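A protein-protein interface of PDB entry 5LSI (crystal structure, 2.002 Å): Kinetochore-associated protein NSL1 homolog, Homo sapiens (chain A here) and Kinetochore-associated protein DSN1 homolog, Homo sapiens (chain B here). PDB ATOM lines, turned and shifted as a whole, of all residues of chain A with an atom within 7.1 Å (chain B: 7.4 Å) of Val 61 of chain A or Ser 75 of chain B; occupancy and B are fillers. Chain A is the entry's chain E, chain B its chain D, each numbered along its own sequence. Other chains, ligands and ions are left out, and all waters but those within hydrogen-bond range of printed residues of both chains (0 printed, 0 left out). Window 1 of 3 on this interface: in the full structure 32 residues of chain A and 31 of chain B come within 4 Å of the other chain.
Hydrophobic or aromatic side chains of chain A that line the printed part of chain B: Val 15, Met 26, Phe 57, Ala 60, Val 61 and Ile 65.
Of the 19 printed residues of chain B, 10 touch a printed residue of chain A.
Hydrophobic or aromatic side chains of chain B within 4 Å of the printed part of chain A: Ile 51, Leu 54, Leu 68, Leu 71, Leu 72 and Phe 78.
Among the printed residues, no Asp or Glu carboxylate lies within 4 Å of a Lys or Arg side-chain nitrogen of the other chain.
Val 15 of chain A touches Leu 68 of chain B (CG1 to CB, 3.9 Å).
Leu 72 of chain B touches Met 26 of chain A (CD2 to SD, 3.6 Å).
CG2 of Thr 56 of chain A touches CB of Ser 79 of chain B, at 3.7 Å.
Ser 75 of chain B touches Phe 57 of chain A (C to CD1, 3.7 Å).
N of Phe 57 of chain A touches CB of Ser 79 of chain B, 3.9 Å away.
Ile 51 of chain B touches Ala 60 of chain A (CD1 to CB, 3.8 Å).
Ala 60 of chain A touches Leu 54 of chain B (CB to CD1, 3.8 Å).
Leu 71 of chain B touches Val 61 of chain A (CD2 to O, 3.8 Å).
OG of Ser 75 of chain B touches CG2 of Val 61 of chain A, at 3.3 Å.
CB of Leu 54 of chain B touches ND2 of Asn 64 of chain A, 3.6 Å away.
The side-chain hydroxyl of Ser 55 of chain B is in hydrogen-bond range of the side-chain amide oxygen of Asn 64 of chain A.
The backbone carbonyl oxygen of Ile 51 of chain B sits at hydrogen-bond distance from the side-chain amide nitrogen of Asn 64 of chain A (3.1 Å).
Val 61 of chain A touches two residues of chain B.
Of the printed residues of chain A, Leu 68 of chain B touches Val 15 (3.9 Å) and Met 26 (3.9 Å).
Of the printed residues of chain B, Ala 53 of chain A touches Ser 79.
Of the printed residues of chain B, Thr 56 of chain A touches Phe 78 and Ser 79.
Printed residues of chain A within 4 Å of Phe 76 of chain B: Phe 57 (3.6 Å).
Printed residues of chain A within 4 Å of Ser 55 of chain B: Asn 64 (2.7 Å).
Trp 72 of chain A touches none of the printed residues of chain B.
The nearest residue of chain B that does not touch Val 61 of chain A is Leu 72 of chain B (4.2 Å).
The backbone carbonyl oxygen (O) of Leu 71 of chain B sits at hydrogen-bond distance from the side-chain hydroxyl (OG) of Ser 75 of chain B (2.8 Å).
The backbone carbonyl oxygen of Val 15 of chain A sits at hydrogen-bond distance from the backbone NH of Ser 66 of chain A, 2.9 Å away.
The backbone carbonyl oxygen (O) of Asn 64 of chain A lies within hydrogen-bond range of the backbone NH (N) of Val 15 of chain A.
The side-chain amide nitrogen of Asn 64 of chain A lies within hydrogen-bond range of the backbone carbonyl oxygen of Ala 60 of chain A (2.7 Å).
The backbone carbonyl oxygen (O) of Phe 76 of chain B sits at hydrogen-bond distance from the side-chain hydroxyl (OG) of Ser 79 of chain B, 3.0 Å away.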
ATOM      1  N   VAL A  15      23.640  15.376 -15.716  1.00  0.00           N
ATOM      2  CA  VAL A  15      24.599  15.245 -14.626  1.00  0.00           C
ATOM      3  C   VAL A  15      24.725  16.584 -13.911  1.00  0.00           C
ATOM      4  O   VAL A  15      24.984  17.618 -14.538  1.00  0.00           O
ATOM      5  CB  VAL A  15      25.953  14.756 -15.157  1.00  0.00           C
ATOM      6  CG1 VAL A  15      26.922  14.510 -14.010  1.00  0.00           C
ATOM      7  CG2 VAL A  15      25.766  13.498 -15.988  1.00  0.00           C
ATOM      8  N   VAL A  23      34.727  21.232 -15.728  1.00  0.00           N
ATOM      9  CA  VAL A  23      34.226  20.462 -16.864  1.00  0.00           C
ATOM     10  C   VAL A  23      35.022  20.793 -18.119  1.00  0.00           C
ATOM     11  O   VAL A  23      35.395  19.897 -18.889  1.00  0.00           O
ATOM     12  CB  VAL A  23      32.721  20.717 -17.063  1.00  0.00           C
ATOM     13  CG1 VAL A  23      32.222  20.027 -18.330  1.00  0.00           C
ATOM     14  CG2 VAL A  23      31.934  20.247 -15.851  1.00  0.00           C
ATOM     15  N   MET A  26      38.317  19.000 -17.962  1.00  0.00           N
ATOM     16  CA  MET A  26      38.094  17.588 -18.260  1.00  0.00           C
ATOM     17  C   MET A  26      37.903  17.356 -19.756  1.00  0.00           C
ATOM     18  O   MET A  26      38.444  16.396 -20.317  1.00  0.00           O
ATOM     19  CB  MET A  26      36.879  17.088 -17.481  1.00  0.00           C
ATOM     20  CG  MET A  26      36.330  15.756 -17.958  1.00  0.00           C
ATOM     21  SD  MET A  26      34.659  15.456 -17.343  1.00  0.00           S
ATOM     22  CE  MET A  26      33.742  16.760 -18.159  1.00  0.00           C
ATOM     23  N   LEU A  27      37.135  18.227 -20.420  1.00  0.00           N
ATOM     24  CA  LEU A  27      36.933  18.090 -21.860  1.00  0.00           C
ATOM     25  C   LEU A  27      38.236  18.287 -22.626  1.00  0.00           C
ATOM     26  O   LEU A  27      38.465  17.634 -23.652  1.00  0.00           O
ATOM     27  CB  LEU A  27      35.875  19.084 -22.342  1.00  0.00           C
ATOM     28  CG  LEU A  27      34.450  18.822 -21.844  1.00  0.00           C
ATOM     29  CD1 LEU A  27      33.487  19.871 -22.377  1.00  0.00           C
ATOM     30  CD2 LEU A  27      33.989  17.429 -22.229  1.00  0.00           C
ATOM     31  N   ALA A  53      34.062  16.858 -35.040  1.00  0.00           N
ATOM     32  CA  ALA A  53      33.969  15.815 -34.020  1.00  0.00           C
ATOM     33  C   ALA A  53      34.227  16.370 -32.626  1.00  0.00           C
ATOM     34  O   ALA A  53      33.548  15.993 -31.665  1.00  0.00           O
ATOM     35  CB  ALA A  53      34.949  14.683 -34.331  1.00  0.00           C
ATOM     36  N   TRP A  55      33.712  19.480 -31.577  1.00  0.00           N
ATOM     37  CA  TRP A  55      32.580  20.324 -31.202  1.00  0.00           C
ATOM     38  C   TRP A  55      31.342  19.487 -30.895  1.00  0.00           C
ATOM     39  O   TRP A  55      30.578  19.810 -29.980  1.00  0.00           O
ATOM     40  CB  TRP A  55      32.305  21.332 -32.322  1.00  0.00           C
ATOM     41  CG  TRP A  55      31.042  22.110 -32.158  1.00  0.00           C
ATOM     42  CD1 TRP A  55      30.685  22.895 -31.093  1.00  0.00           C
ATOM     43  CD2 TRP A  55      29.961  22.187 -33.091  1.00  0.00           C
ATOM     44  NE1 TRP A  55      29.439  23.452 -31.312  1.00  0.00           N
ATOM     45  CE2 TRP A  55      28.976  23.030 -32.533  1.00  0.00           C
ATOM     46  CE3 TRP A  55      29.731  21.625 -34.349  1.00  0.00           C
ATOM     47  CZ2 TRP A  55      27.778  23.320 -33.193  1.00  0.00           C
ATOM     48  CZ3 TRP A  55      28.543  21.913 -35.003  1.00  0.00           C
ATOM     49  CH2 TRP A  55      27.582  22.753 -34.426  1.00  0.00           C
ATOM     50  N   THR A  56      31.127  18.407 -31.649  1.00  0.00           N
ATOM     51  CA  THR A  56      30.045  17.480 -31.329  1.00  0.00           C
ATOM     52  C   THR A  56      30.277  16.827 -29.976  1.00  0.00           C
ATOM     53  O   THR A  56      29.345  16.690 -29.175  1.00  0.00           O
ATOM     54  CB  THR A  56      29.927  16.414 -32.419  1.00  0.00           C
ATOM     55  OG1 THR A  56      29.632  17.042 -33.673  1.00  0.00           O
ATOM     56  CG2 THR A  56      28.830  15.426 -32.082  1.00  0.00           C
ATOM     57  N   PHE A  57      31.519  16.427 -29.700  1.00  0.00           N
ATOM     58  CA  PHE A  57      31.839  15.801 -28.420  1.00  0.00           C
ATOM     59  C   PHE A  57      31.575  16.756 -27.263  1.00  0.00           C
ATOM     60  O   PHE A  57      30.897  16.403 -26.292  1.00  0.00           O
ATOM     61  CB  PHE A  57      33.295  15.334 -28.420  1.00  0.00           C
ATOM     62  CG  PHE A  57      33.791  14.886 -27.074  1.00  0.00           C
ATOM     63  CD1 PHE A  57      33.339  13.705 -26.511  1.00  0.00           C
ATOM     64  CD2 PHE A  57      34.720  15.644 -26.377  1.00  0.00           C
ATOM     65  CE1 PHE A  57      33.796  13.290 -25.271  1.00  0.00           C
ATOM     66  CE2 PHE A  57      35.186  15.235 -25.138  1.00  0.00           C
ATOM     67  CZ  PHE A  57      34.720  14.061 -24.583  1.00  0.00           C
ATOM     68  N   GLU A  58      32.094  17.982 -27.356  1.00  0.00           N
ATOM     69  CA  GLU A  58      31.904  18.943 -26.273  1.00  0.00           C
ATOM     70  C   GLU A  58      30.441  19.340 -26.126  1.00  0.00           C
ATOM     71  O   GLU A  58      29.955  19.530 -25.006  1.00  0.00           O
ATOM     72  CB  GLU A  58      32.781  20.173 -26.506  1.00  0.00           C
ATOM     73  CG  GLU A  58      34.264  19.894 -26.342  1.00  0.00           C
ATOM     74  CD  GLU A  58      35.132  21.084 -26.708  1.00  0.00           C
ATOM     75  OE1 GLU A  58      34.637  21.995 -27.410  1.00  0.00           O
ATOM     76  OE2 GLU A  58      36.311  21.103 -26.294  1.00  0.00           O
ATOM     77  N   SER A  59      29.721  19.470 -27.243  1.00  0.00           N
ATOM     78  CA  SER A  59      28.303  19.815 -27.167  1.00  0.00           C
ATOM     79  C   SER A  59      27.496  18.723 -26.479  1.00  0.00           C
ATOM     80  O   SER A  59      26.630  19.016 -25.649  1.00  0.00           O
ATOM     81  CB  SER A  59      27.744  20.081 -28.563  1.00  0.00           C
ATOM     82  OG  SER A  59      28.327  21.242 -29.119  1.00  0.00           O
ATOM     83  N   ALA A  60      27.768  17.457 -26.803  1.00  0.00           N
ATOM     84  CA  ALA A  60      27.011  16.367 -26.197  1.00  0.00           C
ATOM     85  C   ALA A  60      27.204  16.336 -24.688  1.00  0.00           C
ATOM     86  O   ALA A  60      26.259  16.058 -23.940  1.00  0.00           O
ATOM     87  CB  ALA A  60      27.417  15.031 -26.816  1.00  0.00           C
ATOM     88  N   VAL A  61      28.423  16.616 -24.220  1.00  0.00           N
ATOM     89  CA  VAL A  61      28.669  16.649 -22.781  1.00  0.00           C
ATOM     90  C   VAL A  61      27.984  17.858 -22.158  1.00  0.00           C
ATOM     91  O   VAL A  61      27.272  17.742 -21.155  1.00  0.00           O
ATOM     92  CB  VAL A  61      30.182  16.648 -22.489  1.00  0.00           C
ATOM     93  CG1 VAL A  61      30.439  16.867 -21.006  1.00  0.00           C
ATOM     94  CG2 VAL A  61      30.810  15.343 -22.939  1.00  0.00           C
ATOM     95  N   GLN A  62      28.176  19.036 -22.759  1.00  0.00           N
ATOM     96  CA  GLN A  62      27.660  20.269 -22.171  1.00  0.00           C
ATOM     97  C   GLN A  62      26.136  20.275 -22.115  1.00  0.00           C
ATOM     98  O   GLN A  62      25.547  20.740 -21.131  1.00  0.00           O
ATOM     99  CB  GLN A  62      28.174  21.473 -22.956  1.00  0.00           C
ATOM    100  CG  GLN A  62      29.659  21.730 -22.775  1.00  0.00           C
ATOM    101  CD  GLN A  62      30.205  22.710 -23.792  1.00  0.00           C
ATOM    102  OE1 GLN A  62      29.455  23.282 -24.583  1.00  0.00           O
ATOM    103  NE2 GLN A  62      31.517  22.912 -23.777  1.00  0.00           N
ATOM    104  N   GLU A  63      25.473  19.772 -23.159  1.00  0.00           N
ATOM    105  CA  GLU A  63      24.014  19.770 -23.155  1.00  0.00           C
ATOM    106  C   GLU A  63      23.430  18.716 -22.224  1.00  0.00           C
ATOM    107  O   GLU A  63      22.216  18.725 -21.991  1.00  0.00           O
ATOM    108  CB  GLU A  63      23.476  19.559 -24.571  1.00  0.00           C
ATOM    109  CG  GLU A  63      24.000  20.556 -25.586  1.00  0.00           C
ATOM    110  CD  GLU A  63      22.900  21.179 -26.413  1.00  0.00           C
ATOM    111  OE1 GLU A  63      21.916  21.664 -25.816  1.00  0.00           O
ATOM    112  OE2 GLU A  63      23.019  21.179 -27.658  1.00  0.00           O
ATOM    113  N   ASN A  64      24.256  17.821 -21.680  1.00  0.00           N
ATOM    114  CA  ASN A  64      23.791  16.760 -20.797  1.00  0.00           C
ATOM    115  C   ASN A  64      24.241  16.953 -19.354  1.00  0.00           C
ATOM    116  O   ASN A  64      24.184  16.011 -18.557  1.00  0.00           O
ATOM    117  CB  ASN A  64      24.252  15.400 -21.318  1.00  0.00           C
ATOM    118  CG  ASN A  64      23.370  14.885 -22.424  1.00  0.00           C
ATOM    119  OD1 ASN A  64      22.288  14.360 -22.168  1.00  0.00           O
ATOM    120  ND2 ASN A  64      23.819  15.042 -23.664  1.00  0.00           N
ATOM    121  N   ILE A  65      24.695  18.155 -19.000  1.00  0.00           N
ATOM    122  CA  ILE A  65      24.997  18.489 -17.617  1.00  0.00           C
ATOM    123  C   ILE A  65      24.275  19.783 -17.274  1.00  0.00           C
ATOM    124  O   ILE A  65      23.867  20.548 -18.150  1.00  0.00           O
ATOM    125  CB  ILE A  65      26.514  18.636 -17.338  1.00  0.00           C
ATOM    126  CG1 ILE A  65      27.053  19.941 -17.923  1.00  0.00           C
ATOM    127  CG2 ILE A  65      27.292  17.457 -17.894  1.00  0.00           C
ATOM    128  CD1 ILE A  65      28.554  20.106 -17.759  1.00  0.00           C
ATOM    129  N   SER A  66      24.107  20.008 -15.979  1.00  0.00           N
ATOM    130  CA  SER A  66      23.673  21.292 -15.458  1.00  0.00           C
ATOM    131  C   SER A  66      24.784  21.867 -14.591  1.00  0.00           C
ATOM    132  O   SER A  66      25.528  21.129 -13.939  1.00  0.00           O
ATOM    133  CB  SER A  66      22.377  21.164 -14.647  1.00  0.00           C
ATOM    134  OG  SER A  66      22.549  20.283 -13.549  1.00  0.00           O
ATOM    135  N   TRP A  72      24.190  24.992 -19.328  1.00  0.00           N
ATOM    136  CA  TRP A  72      25.601  25.345 -19.468  1.00  0.00           C
ATOM    137  C   TRP A  72      25.771  26.768 -19.986  1.00  0.00           C
ATOM    138  O   TRP A  72      26.509  27.571 -19.404  1.00  0.00           O
ATOM    139  CB  TRP A  72      26.287  24.345 -20.399  1.00  0.00           C
ATOM    140  CG  TRP A  72      27.690  24.708 -20.795  1.00  0.00           C
ATOM    141  CD1 TRP A  72      28.070  25.533 -21.814  1.00  0.00           C
ATOM    142  CD2 TRP A  72      28.898  24.227 -20.197  1.00  0.00           C
ATOM    143  NE1 TRP A  72      29.442  25.606 -21.878  1.00  0.00           N
ATOM    144  CE2 TRP A  72      29.972  24.810 -20.897  1.00  0.00           C
ATOM    145  CE3 TRP A  72      29.176  23.362 -19.137  1.00  0.00           C
ATOM    146  CZ2 TRP A  72      31.298  24.560 -20.568  1.00  0.00           C
ATOM    147  CZ3 TRP A  72      30.495  23.115 -18.814  1.00  0.00           C
ATOM    148  CH2 TRP A  72      31.539  23.711 -19.526  1.00  0.00           C
ATOM    149  N   ILE B  51      19.302  15.429 -28.072  1.00  0.00           N
ATOM    150  CA  ILE B  51      20.662  15.123 -27.639  1.00  0.00           C
ATOM    151  C   ILE B  51      20.717  14.802 -26.149  1.00  0.00           C
ATOM    152  O   ILE B  51      21.659  14.139 -25.699  1.00  0.00           O
ATOM    153  CB  ILE B  51      21.599  16.288 -28.008  1.00  0.00           C
ATOM    154  CG1 ILE B  51      22.849  15.775 -28.730  1.00  0.00           C
ATOM    155  CG2 ILE B  51      21.976  17.105 -26.784  1.00  0.00           C
ATOM    156  CD1 ILE B  51      23.774  14.950 -27.868  1.00  0.00           C
ATOM    157  N   LEU B  54      21.272  11.211 -24.066  1.00  0.00           N
ATOM    158  CA  LEU B  54      22.505  10.608 -23.574  1.00  0.00           C
ATOM    159  C   LEU B  54      22.485  10.465 -22.058  1.00  0.00           C
ATOM    160  O   LEU B  54      22.761   9.386 -21.524  1.00  0.00           O
ATOM    161  CB  LEU B  54      23.714  11.429 -24.025  1.00  0.00           C
ATOM    162  CG  LEU B  54      24.021  11.422 -25.524  1.00  0.00           C
ATOM    163  CD1 LEU B  54      25.419  11.951 -25.763  1.00  0.00           C
ATOM    164  CD2 LEU B  54      23.879  10.027 -26.109  1.00  0.00           C
ATOM    165  N   SER B  55      22.164  11.546 -21.341  1.00  0.00           N
ATOM    166  CA  SER B  55      22.128  11.465 -19.885  1.00  0.00           C
ATOM    167  C   SER B  55      20.862  10.783 -19.386  1.00  0.00           C
ATOM    168  O   SER B  55      20.873  10.174 -18.312  1.00  0.00           O
ATOM    169  CB  SER B  55      22.261  12.856 -19.262  1.00  0.00           C
ATOM    170  OG  SER B  55      21.239  13.729 -19.707  1.00  0.00           O
ATOM    171  N   ILE B  58      21.563   7.061 -18.803  1.00  0.00           N
ATOM    172  CA  ILE B  58      22.553   6.663 -17.808  1.00  0.00           C
ATOM    173  C   ILE B  58      21.852   6.547 -16.463  1.00  0.00           C
ATOM    174  O   ILE B  58      21.177   7.486 -16.026  1.00  0.00           O
ATOM    175  CB  ILE B  58      23.730   7.654 -17.755  1.00  0.00           C
ATOM    176  CG1 ILE B  58      24.445   7.690 -19.109  1.00  0.00           C
ATOM    177  CG2 ILE B  58      24.713   7.263 -16.664  1.00  0.00           C
ATOM    178  CD1 ILE B  58      25.472   8.799 -19.239  1.00  0.00           C
ATOM    179  N   LEU B  68      28.936  10.991 -14.810  1.00  0.00           N
ATOM    180  CA  LEU B  68      29.741  11.873 -15.649  1.00  0.00           C
ATOM    181  C   LEU B  68      30.772  11.082 -16.443  1.00  0.00           C
ATOM    182  O   LEU B  68      30.972  11.335 -17.636  1.00  0.00           O
ATOM    183  CB  LEU B  68      30.423  12.940 -14.793  1.00  0.00           C
ATOM    184  CG  LEU B  68      31.266  13.948 -15.573  1.00  0.00           C
ATOM    185  CD1 LEU B  68      30.421  14.630 -16.633  1.00  0.00           C
ATOM    186  CD2 LEU B  68      31.887  14.972 -14.635  1.00  0.00           C
ATOM    187  N   GLY B  69      31.433  10.118 -15.799  1.00  0.00           N
ATOM    188  CA  GLY B  69      32.342   9.247 -16.530  1.00  0.00           C
ATOM    189  C   GLY B  69      31.654   8.518 -17.668  1.00  0.00           C
ATOM    190  O   GLY B  69      32.190   8.432 -18.775  1.00  0.00           O
ATOM    191  N   CYS B  70      30.452   7.988 -17.414  1.00  0.00           N
ATOM    192  CA  CYS B  70      29.683   7.349 -18.479  1.00  0.00           C
ATOM    193  C   CYS B  70      29.333   8.341 -19.579  1.00  0.00           C
ATOM    194  O   CYS B  70      29.442   8.023 -20.769  1.00  0.00           O
ATOM    195  CB  CYS B  70      28.409   6.725 -17.910  1.00  0.00           C
ATOM    196  SG  CYS B  70      28.701   5.365 -16.775  1.00  0.00           S
ATOM    197  N   LEU B  71      28.905   9.548 -19.199  1.00  0.00           N
ATOM    198  CA  LEU B  71      28.536  10.553 -20.193  1.00  0.00           C
ATOM    199  C   LEU B  71      29.708  10.891 -21.107  1.00  0.00           C
ATOM    200  O   LEU B  71      29.516  11.160 -22.298  1.00  0.00           O
ATOM    201  CB  LEU B  71      28.020  11.814 -19.498  1.00  0.00           C
ATOM    202  CG  LEU B  71      27.707  12.978 -20.443  1.00  0.00           C
ATOM    203  CD1 LEU B  71      26.584  12.589 -21.406  1.00  0.00           C
ATOM    204  CD2 LEU B  71      27.344  14.220 -19.663  1.00  0.00           C
ATOM    205  N   LEU B  72      30.931  10.891 -20.566  1.00  0.00           N
ATOM    206  CA  LEU B  72      32.101  11.143 -21.402  1.00  0.00           C
ATOM    207  C   LEU B  72      32.218  10.105 -22.510  1.00  0.00           C
ATOM    208  O   LEU B  72      32.507  10.448 -23.663  1.00  0.00           O
ATOM    209  CB  LEU B  72      33.369  11.152 -20.547  1.00  0.00           C
ATOM    210  CG  LEU B  72      33.520  12.294 -19.541  1.00  0.00           C
ATOM    211  CD1 LEU B  72      34.774  12.102 -18.701  1.00  0.00           C
ATOM    212  CD2 LEU B  72      33.557  13.633 -20.259  1.00  0.00           C
ATOM    213  N   LEU B  73      31.987   8.833 -22.185  1.00  0.00           N
ATOM    214  CA  LEU B  73      32.120   7.782 -23.188  1.00  0.00           C
ATOM    215  C   LEU B  73      30.976   7.820 -24.193  1.00  0.00           C
ATOM    216  O   LEU B  73      31.198   7.653 -25.399  1.00  0.00           O
ATOM    217  CB  LEU B  73      32.186   6.414 -22.514  1.00  0.00           C
ATOM    218  CG  LEU B  73      32.356   5.269 -23.510  1.00  0.00           C
ATOM    219  CD1 LEU B  73      33.824   5.113 -23.895  1.00  0.00           C
ATOM    220  CD2 LEU B  73      31.775   3.970 -22.964  1.00  0.00           C
ATOM    221  N   SER B  74      29.745   8.023 -23.718  1.00  0.00           N
ATOM    222  CA  SER B  74      28.607   8.116 -24.627  1.00  0.00           C
ATOM    223  C   SER B  74      28.782   9.264 -25.611  1.00  0.00           C
ATOM    224  O   SER B  74      28.490   9.120 -26.804  1.00  0.00           O
ATOM    225  CB  SER B  74      27.312   8.292 -23.832  1.00  0.00           C
ATOM    226  OG  SER B  74      27.113   7.208 -22.946  1.00  0.00           O
ATOM    227  N   SER B  75      29.261  10.412 -25.131  1.00  0.00           N
ATOM    228  CA  SER B  75      29.482  11.552 -26.014  1.00  0.00           C
ATOM    229  C   SER B  75      30.559  11.249 -27.047  1.00  0.00           C
ATOM    230  O   SER B  75      30.433  11.627 -28.219  1.00  0.00           O
ATOM    231  CB  SER B  75      29.858  12.782 -25.193  1.00  0.00           C
ATOM    232  OG  SER B  75      28.863  13.058 -24.223  1.00  0.00           O
ATOM    233  N   PHE B  76      31.633  10.579 -26.630  1.00  0.00           N
ATOM    234  CA  PHE B  76      32.661  10.179 -27.584  1.00  0.00           C
ATOM    235  C   PHE B  76      32.073   9.279 -28.663  1.00  0.00           C
ATOM    236  O   PHE B  76      32.248   9.527 -29.861  1.00  0.00           O
ATOM    237  CB  PHE B  76      33.801   9.474 -26.851  1.00  0.00           C
ATOM    238  CG  PHE B  76      35.008   9.223 -27.705  1.00  0.00           C
ATOM    239  CD1 PHE B  76      35.388   7.933 -28.033  1.00  0.00           C
ATOM    240  CD2 PHE B  76      35.762  10.280 -28.185  1.00  0.00           C
ATOM    241  CE1 PHE B  76      36.501   7.703 -28.818  1.00  0.00           C
ATOM    242  CE2 PHE B  76      36.872  10.054 -28.970  1.00  0.00           C
ATOM    243  CZ  PHE B  76      37.241   8.764 -29.287  1.00  0.00           C
ATOM    244  N   GLN B  77      31.346   8.237 -28.249  1.00  0.00           N
ATOM    245  CA  GLN B  77      30.720   7.333 -29.209  1.00  0.00           C
ATOM    246  C   GLN B  77      29.692   8.064 -30.066  1.00  0.00           C
ATOM    247  O   GLN B  77      29.539   7.764 -31.257  1.00  0.00           O
ATOM    248  CB  GLN B  77      30.077   6.158 -28.469  1.00  0.00           C
ATOM    249  CG  GLN B  77      31.091   5.261 -27.768  1.00  0.00           C
ATOM    250  CD  GLN B  77      30.471   4.387 -26.689  1.00  0.00           C
ATOM    251  OE1 GLN B  77      29.435   4.727 -26.116  1.00  0.00           O
ATOM    252  NE2 GLN B  77      31.106   3.253 -26.409  1.00  0.00           N
ATOM    253  N   PHE B  78      28.981   9.029 -29.481  1.00  0.00           N
ATOM    254  CA  PHE B  78      28.019   9.811 -30.252  1.00  0.00           C
ATOM    255  C   PHE B  78      28.708  10.574 -31.382  1.00  0.00           C
ATOM    256  O   PHE B  78      28.256  10.541 -32.532  1.00  0.00           O
ATOM    257  CB  PHE B  78      27.264  10.767 -29.329  1.00  0.00           C
ATOM    258  CG  PHE B  78      26.196  11.558 -30.023  1.00  0.00           C
ATOM    259  CD1 PHE B  78      24.948  11.000 -30.257  1.00  0.00           C
ATOM    260  CD2 PHE B  78      26.430  12.861 -30.431  1.00  0.00           C
ATOM    261  CE1 PHE B  78      23.957  11.726 -30.894  1.00  0.00           C
ATOM    262  CE2 PHE B  78      25.443  13.592 -31.071  1.00  0.00           C
ATOM    263  CZ  PHE B  78      24.204  13.021 -31.302  1.00  0.00           C
ATOM    264  N   SER B  79      29.819  11.249 -31.082  1.00  0.00           N
ATOM    265  CA  SER B  79      30.500  12.008 -32.128  1.00  0.00           C
ATOM    266  C   SER B  79      31.124  11.087 -33.171  1.00  0.00           C
ATOM    267  O   SER B  79      31.251  11.475 -34.339  1.00  0.00           O
ATOM    268  CB  SER B  79      31.558  12.932 -31.518  1.00  0.00           C
ATOM    269  OG  SER B  79      32.681  12.206 -31.056  1.00  0.00           O
ATOM    270  N   ILE B  80      31.511   9.872 -32.778  1.00  0.00           N
ATOM    271  CA  ILE B  80      31.972   8.885 -33.754  1.00  0.00           C
ATOM    272  C   ILE B  80      30.862   8.563 -34.746  1.00  0.00           C
ATOM    273  O   ILE B  80      31.071   8.561 -35.965  1.00  0.00           O
ATOM    274  CB  ILE B  80      32.458   7.609 -33.045  1.00  0.00           C
ATOM    275  CG1 ILE B  80      33.661   7.907 -32.159  1.00  0.00           C
ATOM    276  CG2 ILE B  80      32.810   6.542 -34.066  1.00  0.00           C
ATOM    277  CD1 ILE B  80      34.767   8.537 -32.903  1.00  0.00           C
ATOM    278  N   GLN B  81      29.660   8.289 -34.231  1.00  0.00           N
ATOM    279  CA  GLN B  81      28.588   7.770 -35.072  1.00  0.00           C
ATOM    280  C   GLN B  81      28.053   8.818 -36.039  1.00  0.00           C
ATOM    281  O   GLN B  81      27.531   8.461 -37.101  1.00  0.00           O
ATOM    282  CB  GLN B  81      27.455   7.232 -34.204  1.00  0.00           C
ATOM    283  CG  GLN B  81      27.798   5.945 -33.474  1.00  0.00           C
ATOM    284  CD  GLN B  81      26.590   5.334 -32.798  1.00  0.00           C
ATOM    285  OE1 GLN B  81      25.536   5.967 -32.700  1.00  0.00           O
ATOM    286  NE2 GLN B  81      26.731   4.096 -32.332  1.00  0.00           N
ATOM    287  N   LEU B 109      39.689   5.450 -23.752  1.00  0.00           N
ATOM    288  CA  LEU B 109      38.985   6.520 -23.055  1.00  0.00           C
ATOM    289  C   LEU B 109      38.308   6.002 -21.794  1.00  0.00           C
ATOM    290  O   LEU B 109      38.311   6.679 -20.760  1.00  0.00           O
ATOM    291  CB  LEU B 109      37.964   7.178 -23.978  1.00  0.00           C
ATOM    292  CG  LEU B 109      37.163   8.293 -23.301  1.00  0.00           C
ATOM    293  CD1 LEU B 109      38.090   9.425 -22.873  1.00  0.00           C
ATOM    294  CD2 LEU B 109      36.076   8.807 -24.220  1.00  0.00           C
